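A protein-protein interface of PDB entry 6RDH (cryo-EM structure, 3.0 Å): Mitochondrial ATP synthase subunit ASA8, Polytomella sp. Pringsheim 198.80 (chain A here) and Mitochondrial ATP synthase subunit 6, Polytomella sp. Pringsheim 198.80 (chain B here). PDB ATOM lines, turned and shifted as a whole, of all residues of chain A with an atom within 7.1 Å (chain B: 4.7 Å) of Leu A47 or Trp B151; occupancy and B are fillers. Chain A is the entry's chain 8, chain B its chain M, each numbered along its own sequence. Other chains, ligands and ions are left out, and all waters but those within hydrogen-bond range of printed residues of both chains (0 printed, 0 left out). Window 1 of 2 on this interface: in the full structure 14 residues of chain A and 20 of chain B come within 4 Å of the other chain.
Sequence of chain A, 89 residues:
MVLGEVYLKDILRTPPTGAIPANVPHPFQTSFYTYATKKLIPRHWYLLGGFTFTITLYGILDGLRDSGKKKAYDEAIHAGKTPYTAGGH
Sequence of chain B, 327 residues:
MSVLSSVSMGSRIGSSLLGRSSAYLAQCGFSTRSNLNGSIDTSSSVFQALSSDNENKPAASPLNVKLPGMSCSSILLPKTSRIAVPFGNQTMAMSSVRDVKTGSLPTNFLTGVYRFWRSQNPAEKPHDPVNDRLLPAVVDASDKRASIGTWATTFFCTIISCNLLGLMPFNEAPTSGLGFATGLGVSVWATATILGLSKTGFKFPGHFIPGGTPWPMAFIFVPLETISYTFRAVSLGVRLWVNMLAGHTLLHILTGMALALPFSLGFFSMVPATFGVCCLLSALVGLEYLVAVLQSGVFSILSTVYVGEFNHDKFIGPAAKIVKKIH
Of chain B, only Trp B151 (3.5 Å), Phe B155 (3.7 Å) and Thr B191 (3.3 Å) come within 4 Å of Leu A47.
Of chain A, only Arg A43 (3.5 Å), His A44 (3.1 Å), Tyr A46 (3.5 Å) and Leu A47 (3.5 Å) come within 4 Å of Trp B151.
Printed residues of chain B within 4 Å of Tyr A46: Trp B151 (3.5 Å) and Thr B191 (3.6 Å).
Printed residues of chain B within 4 Å of Phe A51: Phe B155.
Printed residues of chain A within 4 Å of Ser B147: Arg A43 (3.1 Å).
Thr B153 touches none of the printed residues of chain A.
The nearest printed residue of chain B that does not touch Leu A47 is Thr B154 (5.1 Å).
The nearest residue of chain A that does not touch Trp B151 is Trp A45 (5.6 Å).
The nearest printed residue of chain B that does not touch His A44 is Ser B147 (4.02 Å).
OG of Ser B147 lies within hydrogen-bond range of NH2 of Arg A43 (3.1 Å).
The indole nitrogen of Trp B151 is in hydrogen-bond range of a ring nitrogen (ND1) of His A44 (3.1 Å).
CZ2 of Trp B151 touches O of Arg A43 (3.5 Å).
CD2 of Tyr A46 touches CH2 of Trp B151 (3.5 Å).
O of Tyr A46 touches OG1 of Thr B191, 3.6 Å away.
Leu A47 touches Trp B151.
Phe B155 touches Leu A47 (CE2 to CD2, 3.7 Å).
Leu A47 touches Thr B191.
Phe B155 touches Phe A51 (CZ to CZ, 3.97 Å).
Of the 12 printed residues of chain B, 4 touch a printed residue of chain A.
Hydrophobic or aromatic side chains of chain B that line the printed part of chain A: Trp B151 and Phe B155.
Among the printed residues, 9 pairs touch across the chains.
Among the printed residues, no Asp or Glu carboxylate lies within 4 Å of a Lys or Arg side-chain nitrogen of the other chain.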
ATOM      1  N   LEU A  40      21.464  16.943  24.833  1.00  0.00           N
ATOM      2  CA  LEU A  40      21.334  17.239  23.410  1.00  0.00           C
ATOM      3  C   LEU A  40      20.466  16.216  22.708  1.00  0.00           C
ATOM      4  O   LEU A  40      19.615  16.573  21.895  1.00  0.00           O
ATOM      5  CB  LEU A  40      22.697  17.303  22.749  1.00  0.00           C
ATOM      6  CG  LEU A  40      22.703  17.692  21.288  1.00  0.00           C
ATOM      7  CD1 LEU A  40      22.216  19.094  21.148  1.00  0.00           C
ATOM      8  CD2 LEU A  40      24.089  17.571  20.755  1.00  0.00           C
ATOM      9  N   ARG A  43      16.738  15.919  24.996  1.00  0.00           N
ATOM     10  CA  ARG A  43      15.875  17.092  25.016  1.00  0.00           C
ATOM     11  C   ARG A  43      15.812  17.848  23.703  1.00  0.00           C
ATOM     12  O   ARG A  43      14.789  18.470  23.428  1.00  0.00           O
ATOM     13  CB  ARG A  43      16.311  18.078  26.105  1.00  0.00           C
ATOM     14  CG  ARG A  43      16.478  17.480  27.464  1.00  0.00           C
ATOM     15  CD  ARG A  43      15.134  17.230  28.093  1.00  0.00           C
ATOM     16  NE  ARG A  43      14.563  18.445  28.649  1.00  0.00           N
ATOM     17  CZ  ARG A  43      13.263  18.676  28.729  1.00  0.00           C
ATOM     18  NH1 ARG A  43      12.409  17.783  28.272  1.00  0.00           N
ATOM     19  NH2 ARG A  43      12.818  19.805  29.253  1.00  0.00           N
ATOM     20  N   HIS A  44      16.864  17.821  22.889  1.00  0.00           N
ATOM     21  CA  HIS A  44      16.934  18.636  21.687  1.00  0.00           C
ATOM     22  C   HIS A  44      16.922  17.804  20.417  1.00  0.00           C
ATOM     23  O   HIS A  44      17.331  18.293  19.358  1.00  0.00           O
ATOM     24  CB  HIS A  44      18.181  19.511  21.703  1.00  0.00           C
ATOM     25  CG  HIS A  44      18.316  20.358  22.925  1.00  0.00           C
ATOM     26  ND1 HIS A  44      17.242  20.950  23.544  1.00  0.00           N
ATOM     27  CD2 HIS A  44      19.404  20.713  23.641  1.00  0.00           C
ATOM     28  CE1 HIS A  44      17.661  21.633  24.591  1.00  0.00           C
ATOM     29  NE2 HIS A  44      18.971  21.505  24.671  1.00  0.00           N
ATOM     30  N   TRP A  45      16.468  16.554  20.485  1.00  0.00           N
ATOM     31  CA  TRP A  45      16.445  15.756  19.270  1.00  0.00           C
ATOM     32  C   TRP A  45      15.340  16.194  18.334  1.00  0.00           C
ATOM     33  O   TRP A  45      15.430  15.931  17.139  1.00  0.00           O
ATOM     34  CB  TRP A  45      16.329  14.267  19.588  1.00  0.00           C
ATOM     35  CG  TRP A  45      15.006  13.787  20.076  1.00  0.00           C
ATOM     36  CD1 TRP A  45      14.612  13.659  21.367  1.00  0.00           C
ATOM     37  CD2 TRP A  45      13.915  13.323  19.279  1.00  0.00           C
ATOM     38  NE1 TRP A  45      13.340  13.162  21.428  1.00  0.00           N
ATOM     39  CE2 TRP A  45      12.889  12.953  20.155  1.00  0.00           C
ATOM     40  CE3 TRP A  45      13.700  13.204  17.908  1.00  0.00           C
ATOM     41  CZ2 TRP A  45      11.676  12.465  19.705  1.00  0.00           C
ATOM     42  CZ3 TRP A  45      12.499  12.727  17.472  1.00  0.00           C
ATOM     43  CH2 TRP A  45      11.501  12.369  18.362  1.00  0.00           C
ATOM     44  N   TYR A  46      14.332  16.903  18.842  1.00  0.00           N
ATOM     45  CA  TYR A  46      13.339  17.515  17.971  1.00  0.00           C
ATOM     46  C   TYR A  46      13.953  18.622  17.127  1.00  0.00           C
ATOM     47  O   TYR A  46      13.675  18.713  15.930  1.00  0.00           O
ATOM     48  CB  TYR A  46      12.185  18.070  18.792  1.00  0.00           C
ATOM     49  CG  TYR A  46      11.728  17.197  19.923  1.00  0.00           C
ATOM     50  CD1 TYR A  46      10.770  16.231  19.726  1.00  0.00           C
ATOM     51  CD2 TYR A  46      12.219  17.375  21.197  1.00  0.00           C
ATOM     52  CE1 TYR A  46      10.336  15.449  20.761  1.00  0.00           C
ATOM     53  CE2 TYR A  46      11.802  16.594  22.231  1.00  0.00           C
ATOM     54  CZ  TYR A  46      10.860  15.634  22.009  1.00  0.00           C
ATOM     55  OH  TYR A  46      10.441  14.857  23.056  1.00  0.00           O
ATOM     56  N   LEU A  47      14.801  19.465  17.727  1.00  0.00           N
ATOM     57  CA  LEU A  47      15.500  20.483  16.949  1.00  0.00           C
ATOM     58  C   LEU A  47      16.488  19.875  15.977  1.00  0.00           C
ATOM     59  O   LEU A  47      16.639  20.369  14.858  1.00  0.00           O
ATOM     60  CB  LEU A  47      16.245  21.463  17.840  1.00  0.00           C
ATOM     61  CG  LEU A  47      15.643  22.820  18.139  1.00  0.00           C
ATOM     62  CD1 LEU A  47      16.752  23.700  18.623  1.00  0.00           C
ATOM     63  CD2 LEU A  47      15.032  23.408  16.907  1.00  0.00           C
ATOM     64  N   LEU A  48      17.185  18.818  16.382  1.00  0.00           N
ATOM     65  CA  LEU A  48      18.136  18.207  15.460  1.00  0.00           C
ATOM     66  C   LEU A  48      17.420  17.500  14.316  1.00  0.00           C
ATOM     67  O   LEU A  48      17.883  17.539  13.172  1.00  0.00           O
ATOM     68  CB  LEU A  48      19.049  17.248  16.205  1.00  0.00           C
ATOM     69  CG  LEU A  48      19.892  17.882  17.305  1.00  0.00           C
ATOM     70  CD1 LEU A  48      20.804  16.839  17.885  1.00  0.00           C
ATOM     71  CD2 LEU A  48      20.678  19.063  16.794  1.00  0.00           C
ATOM     72  N   GLY A  49      16.264  16.896  14.591  1.00  0.00           N
ATOM     73  CA  GLY A  49      15.450  16.344  13.526  1.00  0.00           C
ATOM     74  C   GLY A  49      14.872  17.400  12.616  1.00  0.00           C
ATOM     75  O   GLY A  49      14.746  17.175  11.414  1.00  0.00           O
ATOM     76  N   GLY A  50      14.539  18.569  13.161  1.00  0.00           N
ATOM     77  CA  GLY A  50      14.084  19.662  12.321  1.00  0.00           C
ATOM     78  C   GLY A  50      15.170  20.205  11.415  1.00  0.00           C
ATOM     79  O   GLY A  50      14.926  20.488  10.238  1.00  0.00           O
ATOM     80  N   PHE A  51      16.385  20.341  11.940  1.00  0.00           N
ATOM     81  CA  PHE A  51      17.499  20.808  11.124  1.00  0.00           C
ATOM     82  C   PHE A  51      17.863  19.793  10.050  1.00  0.00           C
ATOM     83  O   PHE A  51      18.146  20.173   8.909  1.00  0.00           O
ATOM     84  CB  PHE A  51      18.703  21.118  12.007  1.00  0.00           C
ATOM     85  CG  PHE A  51      18.554  22.373  12.803  1.00  0.00           C
ATOM     86  CD1 PHE A  51      18.035  23.507  12.224  1.00  0.00           C
ATOM     87  CD2 PHE A  51      18.924  22.420  14.128  1.00  0.00           C
ATOM     88  CE1 PHE A  51      17.880  24.662  12.950  1.00  0.00           C
ATOM     89  CE2 PHE A  51      18.771  23.568  14.856  1.00  0.00           C
ATOM     90  CZ  PHE A  51      18.248  24.687  14.265  1.00  0.00           C
ATOM     91  N   THR A  52      17.816  18.499  10.372  1.00  0.00           N
ATOM     92  CA  THR A  52      18.092  17.505   9.341  1.00  0.00           C
ATOM     93  C   THR A  52      16.978  17.417   8.315  1.00  0.00           C
ATOM     94  O   THR A  52      17.262  17.178   7.135  1.00  0.00           O
ATOM     95  CB  THR A  52      18.336  16.134   9.949  1.00  0.00           C
ATOM     96  OG1 THR A  52      17.218  15.764  10.757  1.00  0.00           O
ATOM     97  CG2 THR A  52      19.604  16.142  10.767  1.00  0.00           C
ATOM     98  N   PHE A  53      15.721  17.614   8.723  1.00  0.00           N
ATOM     99  CA  PHE A  53      14.633  17.654   7.755  1.00  0.00           C
ATOM    100  C   PHE A  53      14.801  18.814   6.793  1.00  0.00           C
ATOM    101  O   PHE A  53      14.584  18.658   5.589  1.00  0.00           O
ATOM    102  CB  PHE A  53      13.283  17.761   8.454  1.00  0.00           C
ATOM    103  CG  PHE A  53      12.132  17.967   7.509  1.00  0.00           C
ATOM    104  CD1 PHE A  53      11.630  16.912   6.783  1.00  0.00           C
ATOM    105  CD2 PHE A  53      11.554  19.213   7.346  1.00  0.00           C
ATOM    106  CE1 PHE A  53      10.584  17.092   5.916  1.00  0.00           C
ATOM    107  CE2 PHE A  53      10.508  19.395   6.477  1.00  0.00           C
ATOM    108  CZ  PHE A  53      10.023  18.335   5.766  1.00  0.00           C
ATOM    109  N   ALA B 146       8.659  20.058  26.215  1.00  0.00           N
ATOM    110  CA  ALA B 146       9.790  20.393  25.372  1.00  0.00           C
ATOM    111  C   ALA B 146      10.487  21.630  25.902  1.00  0.00           C
ATOM    112  O   ALA B 146       9.881  22.481  26.553  1.00  0.00           O
ATOM    113  CB  ALA B 146       9.343  20.633  23.938  1.00  0.00           C
ATOM    114  N   SER B 147      11.779  21.734  25.609  1.00  0.00           N
ATOM    115  CA  SER B 147      12.573  22.882  26.033  1.00  0.00           C
ATOM    116  C   SER B 147      12.347  24.040  25.068  1.00  0.00           C
ATOM    117  O   SER B 147      13.239  24.470  24.345  1.00  0.00           O
ATOM    118  CB  SER B 147      14.044  22.511  26.098  1.00  0.00           C
ATOM    119  OG  SER B 147      14.278  21.497  27.047  1.00  0.00           O
ATOM    120  N   ILE B 148      11.120  24.560  25.069  1.00  0.00           N
ATOM    121  CA  ILE B 148      10.814  25.671  24.189  1.00  0.00           C
ATOM    122  C   ILE B 148      11.432  26.950  24.711  1.00  0.00           C
ATOM    123  O   ILE B 148      11.644  27.883  23.937  1.00  0.00           O
ATOM    124  CB  ILE B 148       9.298  25.836  24.006  1.00  0.00           C
ATOM    125  CG1 ILE B 148       8.636  24.481  23.879  1.00  0.00           C
ATOM    126  CG2 ILE B 148       8.992  26.560  22.729  1.00  0.00           C
ATOM    127  CD1 ILE B 148       7.152  24.551  23.925  1.00  0.00           C
ATOM    128  N   GLY B 149      11.730  27.022  26.005  1.00  0.00           N
ATOM    129  CA  GLY B 149      12.457  28.170  26.516  1.00  0.00           C
ATOM    130  C   GLY B 149      13.847  28.259  25.931  1.00  0.00           C
ATOM    131  O   GLY B 149      14.237  29.296  25.399  1.00  0.00           O
ATOM    132  N   THR B 150      14.566  27.133  25.934  1.00  0.00           N
ATOM    133  CA  THR B 150      15.917  27.067  25.393  1.00  0.00           C
ATOM    134  C   THR B 150      15.929  27.232  23.881  1.00  0.00           C
ATOM    135  O   THR B 150      16.775  27.954  23.344  1.00  0.00           O
ATOM    136  CB  THR B 150      16.554  25.742  25.779  1.00  0.00           C
ATOM    137  OG1 THR B 150      16.409  25.540  27.184  1.00  0.00           O
ATOM    138  CG2 THR B 150      18.009  25.746  25.460  1.00  0.00           C
ATOM    139  N   TRP B 151      14.986  26.598  23.179  1.00  0.00           N
ATOM    140  CA  TRP B 151      14.916  26.723  21.725  1.00  0.00           C
ATOM    141  C   TRP B 151      14.535  28.127  21.309  1.00  0.00           C
ATOM    142  O   TRP B 151      15.072  28.656  20.337  1.00  0.00           O
ATOM    143  CB  TRP B 151      13.897  25.761  21.137  1.00  0.00           C
ATOM    144  CG  TRP B 151      14.127  24.340  21.387  1.00  0.00           C
ATOM    145  CD1 TRP B 151      15.269  23.753  21.794  1.00  0.00           C
ATOM    146  CD2 TRP B 151      13.165  23.300  21.255  1.00  0.00           C
ATOM    147  NE1 TRP B 151      15.090  22.409  21.914  1.00  0.00           N
ATOM    148  CE2 TRP B 151      13.798  22.107  21.587  1.00  0.00           C
ATOM    149  CE3 TRP B 151      11.827  23.269  20.872  1.00  0.00           C
ATOM    150  CZ2 TRP B 151      13.146  20.895  21.555  1.00  0.00           C
ATOM    151  CZ3 TRP B 151      11.183  22.069  20.847  1.00  0.00           C
ATOM    152  CH2 TRP B 151      11.838  20.898  21.186  1.00  0.00           C
ATOM    153  N   ALA B 152      13.595  28.739  22.015  1.00  0.00           N
ATOM    154  CA  ALA B 152      13.160  30.073  21.646  1.00  0.00           C
ATOM    155  C   ALA B 152      14.226  31.107  21.921  1.00  0.00           C
ATOM    156  O   ALA B 152      14.383  32.034  21.129  1.00  0.00           O
ATOM    157  CB  ALA B 152      11.878  30.433  22.374  1.00  0.00           C
ATOM    158  N   THR B 153      14.996  30.971  23.003  1.00  0.00           N
ATOM    159  CA  THR B 153      16.077  31.936  23.149  1.00  0.00           C
ATOM    160  C   THR B 153      17.253  31.627  22.242  1.00  0.00           C
ATOM    161  O   THR B 153      17.971  32.557  21.875  1.00  0.00           O
ATOM    162  CB  THR B 153      16.543  32.072  24.595  1.00  0.00           C
ATOM    163  OG1 THR B 153      17.642  32.978  24.640  1.00  0.00           O
ATOM    164  CG2 THR B 153      17.000  30.818  25.132  1.00  0.00           C
ATOM    165  N   THR B 154      17.415  30.374  21.814  1.00  0.00           N
ATOM    166  CA  THR B 154      18.373  30.044  20.764  1.00  0.00           C
ATOM    167  C   THR B 154      18.032  30.761  19.471  1.00  0.00           C
ATOM    168  O   THR B 154      18.887  31.422  18.873  1.00  0.00           O
ATOM    169  CB  THR B 154      18.381  28.538  20.545  1.00  0.00           C
ATOM    170  OG1 THR B 154      19.012  27.904  21.652  1.00  0.00           O
ATOM    171  CG2 THR B 154      19.108  28.172  19.291  1.00  0.00           C
ATOM    172  N   PHE B 155      16.770  30.678  19.055  1.00  0.00           N
ATOM    173  CA  PHE B 155      16.351  31.301  17.806  1.00  0.00           C
ATOM    174  C   PHE B 155      16.320  32.812  17.916  1.00  0.00           C
ATOM    175  O   PHE B 155      16.667  33.502  16.959  1.00  0.00           O
ATOM    176  CB  PHE B 155      14.997  30.761  17.380  1.00  0.00           C
ATOM    177  CG  PHE B 155      15.080  29.422  16.753  1.00  0.00           C
ATOM    178  CD1 PHE B 155      15.839  29.230  15.621  1.00  0.00           C
ATOM    179  CD2 PHE B 155      14.425  28.348  17.302  1.00  0.00           C
ATOM    180  CE1 PHE B 155      15.928  28.001  15.048  1.00  0.00           C
ATOM    181  CE2 PHE B 155      14.523  27.112  16.742  1.00  0.00           C
ATOM    182  CZ  PHE B 155      15.270  26.939  15.609  1.00  0.00           C
ATOM    183  N   THR B 191      10.416  21.073  13.800  1.00  0.00           N
ATOM    184  CA  THR B 191      10.544  20.766  15.221  1.00  0.00           C
ATOM    185  C   THR B 191       9.186  20.611  15.882  1.00  0.00           C
ATOM    186  O   THR B 191       8.969  19.666  16.650  1.00  0.00           O
ATOM    187  CB  THR B 191      11.329  21.870  15.902  1.00  0.00           C
ATOM    188  OG1 THR B 191      12.544  22.075  15.184  1.00  0.00           O
ATOM    189  CG2 THR B 191      11.643  21.501  17.302  1.00  0.00           C
ATOM    190  N   VAL B 307       5.288  25.404  18.685  1.00  0.00           N
ATOM    191  CA  VAL B 307       5.777  24.233  19.394  1.00  0.00           C
ATOM    192  C   VAL B 307       4.930  23.958  20.624  1.00  0.00           C
ATOM    193  O   VAL B 307       4.633  22.802  20.924  1.00  0.00           O
ATOM    194  CB  VAL B 307       7.266  24.401  19.733  1.00  0.00           C
ATOM    195  CG1 VAL B 307       7.781  23.216  20.489  1.00  0.00           C
ATOM    196  CG2 VAL B 307       8.072  24.540  18.468  1.00  0.00           C
